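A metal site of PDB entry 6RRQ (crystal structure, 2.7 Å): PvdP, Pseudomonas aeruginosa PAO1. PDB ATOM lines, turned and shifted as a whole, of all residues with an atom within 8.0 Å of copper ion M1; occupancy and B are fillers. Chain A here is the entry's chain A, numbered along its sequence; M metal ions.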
ATOM      1  N   PHE A 215      -3.783 -20.017 -19.953  1.00  0.00           N
ATOM      2  CA  PHE A 215      -3.935 -21.064 -20.936  1.00  0.00           C
ATOM      3  C   PHE A 215      -2.911 -20.826 -22.044  1.00  0.00           C
ATOM      4  O   PHE A 215      -2.067 -21.685 -22.331  1.00  0.00           O
ATOM      5  CB  PHE A 215      -5.366 -21.104 -21.519  1.00  0.00           C
ATOM      6  CG  PHE A 215      -5.505 -22.013 -22.728  1.00  0.00           C
ATOM      7  CD1 PHE A 215      -5.255 -21.539 -24.021  1.00  0.00           C
ATOM      8  CD2 PHE A 215      -5.862 -23.340 -22.577  1.00  0.00           C
ATOM      9  CE1 PHE A 215      -5.345 -22.379 -25.119  1.00  0.00           C
ATOM     10  CE2 PHE A 215      -5.963 -24.182 -23.684  1.00  0.00           C
ATOM     11  CZ  PHE A 215      -5.710 -23.705 -24.948  1.00  0.00           C
ATOM     12  N   HIS A 216      -2.972 -19.635 -22.641  1.00  0.00           N
ATOM     13  CA  HIS A 216      -2.100 -19.288 -23.759  1.00  0.00           C
ATOM     14  C   HIS A 216      -0.616 -19.462 -23.396  1.00  0.00           C
ATOM     15  O   HIS A 216       0.150 -20.123 -24.155  1.00  0.00           O
ATOM     16  CB  HIS A 216      -2.383 -17.858 -24.202  1.00  0.00           C
ATOM     17  CG  HIS A 216      -1.965 -17.547 -25.609  1.00  0.00           C
ATOM     18  ND1 HIS A 216      -1.935 -16.266 -26.108  1.00  0.00           N
ATOM     19  CD2 HIS A 216      -1.586 -18.355 -26.624  1.00  0.00           C
ATOM     20  CE1 HIS A 216      -1.559 -16.294 -27.373  1.00  0.00           C
ATOM     21  NE2 HIS A 216      -1.328 -17.554 -27.703  1.00  0.00           N
ATOM     22  N   GLN A 217      -0.219 -18.915 -22.246  1.00  0.00           N
ATOM     23  CA  GLN A 217       1.165 -19.067 -21.783  1.00  0.00           C
ATOM     24  C   GLN A 217       1.602 -20.522 -21.616  1.00  0.00           C
ATOM     25  O   GLN A 217       2.682 -20.916 -22.092  1.00  0.00           O
ATOM     26  CB  GLN A 217       1.416 -18.329 -20.464  1.00  0.00           C
ATOM     27  CG  GLN A 217       2.905 -18.067 -20.218  1.00  0.00           C
ATOM     28  CD  GLN A 217       3.202 -17.596 -18.805  1.00  0.00           C
ATOM     29  OE1 GLN A 217       4.322 -17.731 -18.334  1.00  0.00           O
ATOM     30  NE2 GLN A 217       2.196 -17.060 -18.136  1.00  0.00           N
ATOM     31  N   TRP A 219       0.117 -23.376 -22.831  1.00  0.00           N
ATOM     32  CA  TRP A 219       0.065 -24.051 -24.148  1.00  0.00           C
ATOM     33  C   TRP A 219       1.393 -23.919 -24.936  1.00  0.00           C
ATOM     34  O   TRP A 219       1.898 -24.906 -25.475  1.00  0.00           O
ATOM     35  CB  TRP A 219      -1.086 -23.459 -24.990  1.00  0.00           C
ATOM     36  CG  TRP A 219      -1.375 -24.239 -26.185  1.00  0.00           C
ATOM     37  CD1 TRP A 219      -2.242 -25.278 -26.300  1.00  0.00           C
ATOM     38  CD2 TRP A 219      -0.785 -24.069 -27.462  1.00  0.00           C
ATOM     39  NE1 TRP A 219      -2.233 -25.780 -27.565  1.00  0.00           N
ATOM     40  CE2 TRP A 219      -1.329 -25.064 -28.310  1.00  0.00           C
ATOM     41  CE3 TRP A 219       0.166 -23.181 -27.991  1.00  0.00           C
ATOM     42  CZ2 TRP A 219      -0.967 -25.178 -29.643  1.00  0.00           C
ATOM     43  CZ3 TRP A 219       0.523 -23.299 -29.316  1.00  0.00           C
ATOM     44  CH2 TRP A 219      -0.032 -24.307 -30.126  1.00  0.00           C
ATOM     45  N   HIS A 220       1.938 -22.699 -25.008  1.00  0.00           N
ATOM     46  CA  HIS A 220       3.247 -22.453 -25.629  1.00  0.00           C
ATOM     47  C   HIS A 220       4.369 -23.005 -24.775  1.00  0.00           C
ATOM     48  O   HIS A 220       5.243 -23.684 -25.266  1.00  0.00           O
ATOM     49  CB  HIS A 220       3.474 -20.959 -25.879  1.00  0.00           C
ATOM     50  CG  HIS A 220       2.705 -20.431 -27.042  1.00  0.00           C
ATOM     51  ND1 HIS A 220       2.951 -20.847 -28.334  1.00  0.00           N
ATOM     52  CD2 HIS A 220       1.678 -19.553 -27.115  1.00  0.00           C
ATOM     53  CE1 HIS A 220       2.109 -20.220 -29.151  1.00  0.00           C
ATOM     54  NE2 HIS A 220       1.331 -19.445 -28.436  1.00  0.00           N
ATOM     55  N   ARG A 223       4.731 -26.994 -25.123  1.00  0.00           N
ATOM     56  CA  ARG A 223       5.256 -27.449 -26.397  1.00  0.00           C
ATOM     57  C   ARG A 223       6.627 -26.869 -26.682  1.00  0.00           C
ATOM     58  O   ARG A 223       7.524 -27.625 -27.130  1.00  0.00           O
ATOM     59  CB  ARG A 223       4.280 -27.227 -27.546  1.00  0.00           C
ATOM     60  CG  ARG A 223       3.936 -25.801 -27.836  1.00  0.00           C
ATOM     61  CD  ARG A 223       2.626 -25.718 -28.601  1.00  0.00           C
ATOM     62  NE  ARG A 223       2.690 -26.422 -29.879  1.00  0.00           N
ATOM     63  CZ  ARG A 223       3.226 -25.944 -31.008  1.00  0.00           C
ATOM     64  NH1 ARG A 223       3.752 -24.727 -31.069  1.00  0.00           N
ATOM     65  NH2 ARG A 223       3.219 -26.685 -32.102  1.00  0.00           N
ATOM     66  N   PHE A 267      -0.145 -25.832 -33.712  1.00  0.00           N
ATOM     67  CA  PHE A 267      -0.015 -24.386 -33.854  1.00  0.00           C
ATOM     68  C   PHE A 267      -1.097 -23.798 -34.756  1.00  0.00           C
ATOM     69  O   PHE A 267      -1.806 -22.865 -34.349  1.00  0.00           O
ATOM     70  CB  PHE A 267       1.385 -24.021 -34.363  1.00  0.00           C
ATOM     71  CG  PHE A 267       1.452 -22.642 -34.958  1.00  0.00           C
ATOM     72  CD1 PHE A 267       1.459 -21.530 -34.137  1.00  0.00           C
ATOM     73  CD2 PHE A 267       1.481 -22.460 -36.334  1.00  0.00           C
ATOM     74  CE1 PHE A 267       1.487 -20.264 -34.685  1.00  0.00           C
ATOM     75  CE2 PHE A 267       1.514 -21.207 -36.885  1.00  0.00           C
ATOM     76  CZ  PHE A 267       1.530 -20.099 -36.060  1.00  0.00           C
ATOM     77  N   MET A 270      -4.778 -24.502 -33.218  1.00  0.00           N
ATOM     78  CA  MET A 270      -5.087 -23.825 -31.954  1.00  0.00           C
ATOM     79  C   MET A 270      -5.458 -22.390 -32.192  1.00  0.00           C
ATOM     80  O   MET A 270      -6.471 -21.936 -31.703  1.00  0.00           O
ATOM     81  CB  MET A 270      -3.952 -23.900 -30.950  1.00  0.00           C
ATOM     82  CG  MET A 270      -4.394 -23.524 -29.537  1.00  0.00           C
ATOM     83  SD  MET A 270      -4.511 -21.755 -29.262  1.00  0.00           S
ATOM     84  CE  MET A 270      -2.880 -21.378 -28.629  1.00  0.00           C
ATOM     85  N   HIS A 271      -4.637 -21.654 -32.945  1.00  0.00           N
ATOM     86  CA  HIS A 271      -4.920 -20.235 -33.182  1.00  0.00           C
ATOM     87  C   HIS A 271      -6.146 -20.029 -34.064  1.00  0.00           C
ATOM     88  O   HIS A 271      -6.799 -18.993 -33.923  1.00  0.00           O
ATOM     89  CB  HIS A 271      -3.691 -19.541 -33.747  1.00  0.00           C
ATOM     90  CG  HIS A 271      -2.549 -19.533 -32.788  1.00  0.00           C
ATOM     91  ND1 HIS A 271      -1.590 -20.521 -32.781  1.00  0.00           N
ATOM     92  CD2 HIS A 271      -2.277 -18.729 -31.739  1.00  0.00           C
ATOM     93  CE1 HIS A 271      -0.741 -20.286 -31.791  1.00  0.00           C
ATOM     94  NE2 HIS A 271      -1.142 -19.215 -31.134  1.00  0.00           N
ATOM     95  N   MET A 274      -8.845 -20.048 -31.608  1.00  0.00           N
ATOM     96  CA  MET A 274      -8.864 -18.778 -30.883  1.00  0.00           C
ATOM     97  C   MET A 274      -9.446 -17.663 -31.756  1.00  0.00           C
ATOM     98  O   MET A 274     -10.116 -16.754 -31.267  1.00  0.00           O
ATOM     99  CB  MET A 274      -7.458 -18.427 -30.410  1.00  0.00           C
ATOM    100  CG  MET A 274      -7.458 -17.556 -29.160  1.00  0.00           C
ATOM    101  SD  MET A 274      -5.826 -16.904 -28.757  1.00  0.00           S
ATOM    102  CE  MET A 274      -4.968 -18.473 -28.550  1.00  0.00           C
ATOM    103  N   GLU A 371       5.523 -20.958 -37.854  1.00  0.00           N
ATOM    104  CA  GLU A 371       5.583 -20.550 -36.442  1.00  0.00           C
ATOM    105  C   GLU A 371       6.971 -20.046 -36.062  1.00  0.00           C
ATOM    106  O   GLU A 371       7.136 -18.989 -35.477  1.00  0.00           O
ATOM    107  CB  GLU A 371       5.205 -21.656 -35.473  1.00  0.00           C
ATOM    108  CG  GLU A 371       4.978 -21.115 -34.063  1.00  0.00           C
ATOM    109  CD  GLU A 371       4.721 -22.170 -33.008  1.00  0.00           C
ATOM    110  OE1 GLU A 371       4.756 -23.388 -33.310  1.00  0.00           O
ATOM    111  OE2 GLU A 371       4.476 -21.740 -31.855  1.00  0.00           O
ATOM    112  N   HIS A 375       6.320 -16.142 -37.839  1.00  0.00           N
ATOM    113  CA  HIS A 375       5.373 -15.808 -36.754  1.00  0.00           C
ATOM    114  C   HIS A 375       6.027 -15.152 -35.551  1.00  0.00           C
ATOM    115  O   HIS A 375       5.530 -14.149 -35.037  1.00  0.00           O
ATOM    116  CB  HIS A 375       4.594 -17.057 -36.316  1.00  0.00           C
ATOM    117  CG  HIS A 375       3.925 -16.926 -34.993  1.00  0.00           C
ATOM    118  ND1 HIS A 375       4.521 -17.344 -33.816  1.00  0.00           N
ATOM    119  CD2 HIS A 375       2.722 -16.409 -34.645  1.00  0.00           C
ATOM    120  CE1 HIS A 375       3.707 -17.085 -32.808  1.00  0.00           C
ATOM    121  NE2 HIS A 375       2.604 -16.524 -33.285  1.00  0.00           N
ATOM    122  N   HIS A 379       5.444 -11.010 -34.296  1.00  0.00           N
ATOM    123  CA  HIS A 379       5.218 -10.575 -32.900  1.00  0.00           C
ATOM    124  C   HIS A 379       6.141  -9.451 -32.474  1.00  0.00           C
ATOM    125  O   HIS A 379       5.684  -8.393 -32.103  1.00  0.00           O
ATOM    126  CB  HIS A 379       5.314 -11.755 -31.900  1.00  0.00           C
ATOM    127  CG  HIS A 379       4.031 -12.484 -31.697  1.00  0.00           C
ATOM    128  ND1 HIS A 379       3.340 -12.470 -30.502  1.00  0.00           N
ATOM    129  CD2 HIS A 379       3.305 -13.237 -32.548  1.00  0.00           C
ATOM    130  CE1 HIS A 379       2.248 -13.179 -30.632  1.00  0.00           C
ATOM    131  NE2 HIS A 379       2.187 -13.655 -31.867  1.00  0.00           N
ATOM    132  N   ASP A 418       5.208 -12.061 -25.240  1.00  0.00           N
ATOM    133  CA  ASP A 418       4.926 -13.011 -24.176  1.00  0.00           C
ATOM    134  C   ASP A 418       3.513 -13.502 -24.407  1.00  0.00           C
ATOM    135  O   ASP A 418       2.610 -12.680 -24.474  1.00  0.00           O
ATOM    136  CB  ASP A 418       5.054 -12.266 -22.847  1.00  0.00           C
ATOM    137  CG  ASP A 418       4.788 -13.121 -21.642  1.00  0.00           C
ATOM    138  OD1 ASP A 418       4.824 -14.360 -21.727  1.00  0.00           O
ATOM    139  OD2 ASP A 418       4.558 -12.500 -20.578  1.00  0.00           O
ATOM    140  N   PRO A 419       3.321 -14.828 -24.552  1.00  0.00           N
ATOM    141  CA  PRO A 419       1.984 -15.364 -24.859  1.00  0.00           C
ATOM    142  C   PRO A 419       0.917 -15.196 -23.758  1.00  0.00           C
ATOM    143  O   PRO A 419      -0.275 -15.320 -24.041  1.00  0.00           O
ATOM    144  CB  PRO A 419       2.260 -16.831 -25.158  1.00  0.00           C
ATOM    145  CG  PRO A 419       3.539 -17.131 -24.434  1.00  0.00           C
ATOM    146  CD  PRO A 419       4.335 -15.901 -24.629  1.00  0.00           C
ATOM    147  N   PHE A 420       1.354 -14.915 -22.531  1.00  0.00           N
ATOM    148  CA  PHE A 420       0.518 -14.462 -21.411  1.00  0.00           C
ATOM    149  C   PHE A 420      -0.181 -13.122 -21.691  1.00  0.00           C
ATOM    150  O   PHE A 420      -1.260 -12.854 -21.132  1.00  0.00           O
ATOM    151  CB  PHE A 420       1.420 -14.303 -20.170  1.00  0.00           C
ATOM    152  CG  PHE A 420       0.711 -13.821 -18.920  1.00  0.00           C
ATOM    153  CD1 PHE A 420       0.049 -14.720 -18.071  1.00  0.00           C
ATOM    154  CD2 PHE A 420       0.740 -12.472 -18.545  1.00  0.00           C
ATOM    155  CE1 PHE A 420      -0.576 -14.283 -16.917  1.00  0.00           C
ATOM    156  CE2 PHE A 420       0.107 -12.031 -17.394  1.00  0.00           C
ATOM    157  CZ  PHE A 420      -0.549 -12.937 -16.572  1.00  0.00           C
ATOM    158  N   SER A 422       0.259 -11.471 -25.327  1.00  0.00           N
ATOM    159  CA  SER A 422       0.287 -11.054 -26.741  1.00  0.00           C
ATOM    160  C   SER A 422      -1.093 -10.977 -27.400  1.00  0.00           C
ATOM    161  O   SER A 422      -1.398 -10.018 -28.117  1.00  0.00           O
ATOM    162  CB  SER A 422       1.217 -11.946 -27.556  1.00  0.00           C
ATOM    163  OG  SER A 422       0.810 -13.296 -27.440  1.00  0.00           O
ATOM    164  N   HIS A 423      -1.939 -11.983 -27.137  1.00  0.00           N
ATOM    165  CA  HIS A 423      -3.358 -12.022 -27.590  1.00  0.00           C
ATOM    166  C   HIS A 423      -4.234 -10.829 -27.234  1.00  0.00           C
ATOM    167  O   HIS A 423      -5.321 -10.694 -27.787  1.00  0.00           O
ATOM    168  CB  HIS A 423      -4.041 -13.267 -27.044  1.00  0.00           C
ATOM    169  CG  HIS A 423      -4.045 -13.354 -25.548  1.00  0.00           C
ATOM    170  ND1 HIS A 423      -3.032 -13.960 -24.851  1.00  0.00           N
ATOM    171  CD2 HIS A 423      -4.924 -12.893 -24.627  1.00  0.00           C
ATOM    172  CE1 HIS A 423      -3.270 -13.848 -23.551  1.00  0.00           C
ATOM    173  NE2 HIS A 423      -4.428 -13.217 -23.392  1.00  0.00           N
ATOM    174  N   PHE A 428      -2.103  -8.354 -33.050  1.00  0.00           N
ATOM    175  CA  PHE A 428      -2.245  -9.845 -32.980  1.00  0.00           C
ATOM    176  C   PHE A 428      -3.297 -10.478 -33.920  1.00  0.00           C
ATOM    177  O   PHE A 428      -2.991 -11.443 -34.643  1.00  0.00           O
ATOM    178  CB  PHE A 428      -2.592 -10.242 -31.541  1.00  0.00           C
ATOM    179  CG  PHE A 428      -2.519 -11.708 -31.252  1.00  0.00           C
ATOM    180  CD1 PHE A 428      -3.647 -12.519 -31.420  1.00  0.00           C
ATOM    181  CD2 PHE A 428      -1.364 -12.283 -30.744  1.00  0.00           C
ATOM    182  CE1 PHE A 428      -3.619 -13.868 -31.115  1.00  0.00           C
ATOM    183  CE2 PHE A 428      -1.320 -13.641 -30.432  1.00  0.00           C
ATOM    184  CZ  PHE A 428      -2.450 -14.427 -30.616  1.00  0.00           C
ATOM    185  N   HIS A 432      -2.500 -12.959 -37.037  1.00  0.00           N
ATOM    186  CA  HIS A 432      -2.963 -14.334 -36.880  1.00  0.00           C
ATOM    187  C   HIS A 432      -4.089 -14.585 -37.848  1.00  0.00           C
ATOM    188  O   HIS A 432      -4.213 -15.699 -38.341  1.00  0.00           O
ATOM    189  CB  HIS A 432      -3.345 -14.657 -35.455  1.00  0.00           C
ATOM    190  CG  HIS A 432      -2.172 -15.085 -34.633  1.00  0.00           C
ATOM    191  ND1 HIS A 432      -1.600 -16.332 -34.768  1.00  0.00           N
ATOM    192  CD2 HIS A 432      -1.431 -14.411 -33.718  1.00  0.00           C
ATOM    193  CE1 HIS A 432      -0.577 -16.419 -33.941  1.00  0.00           C
ATOM    194  NE2 HIS A 432      -0.433 -15.262 -33.307  1.00  0.00           N
HETATM  195 CU    CU M   1      -0.325 -18.239 -29.396  1.00  0.00          CU
HETATM  196 CU    CU M   2       1.136 -15.644 -32.219  1.00  0.00          CU
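A ring nitrogen (ND1) of His 216 lies within hydrogen-bond range of a ring nitrogen (ND1) of His 423 (2.8 Å). The backbone carbonyl oxygen (O) of Phe 267 sits at hydrogen-bond distance from a ring nitrogen (ND1) of His 271. O of Pro 419 is in hydrogen-bond range of ND1 of His 216, at 2.8 Å.
Copper ion M1 is bound by a ring nitrogen (NE2) of His 216, a ring nitrogen (NE2) of His 271 and a ring nitrogen (NE2) of His 220. Copper ion M1 has three donor atoms within binding distance.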
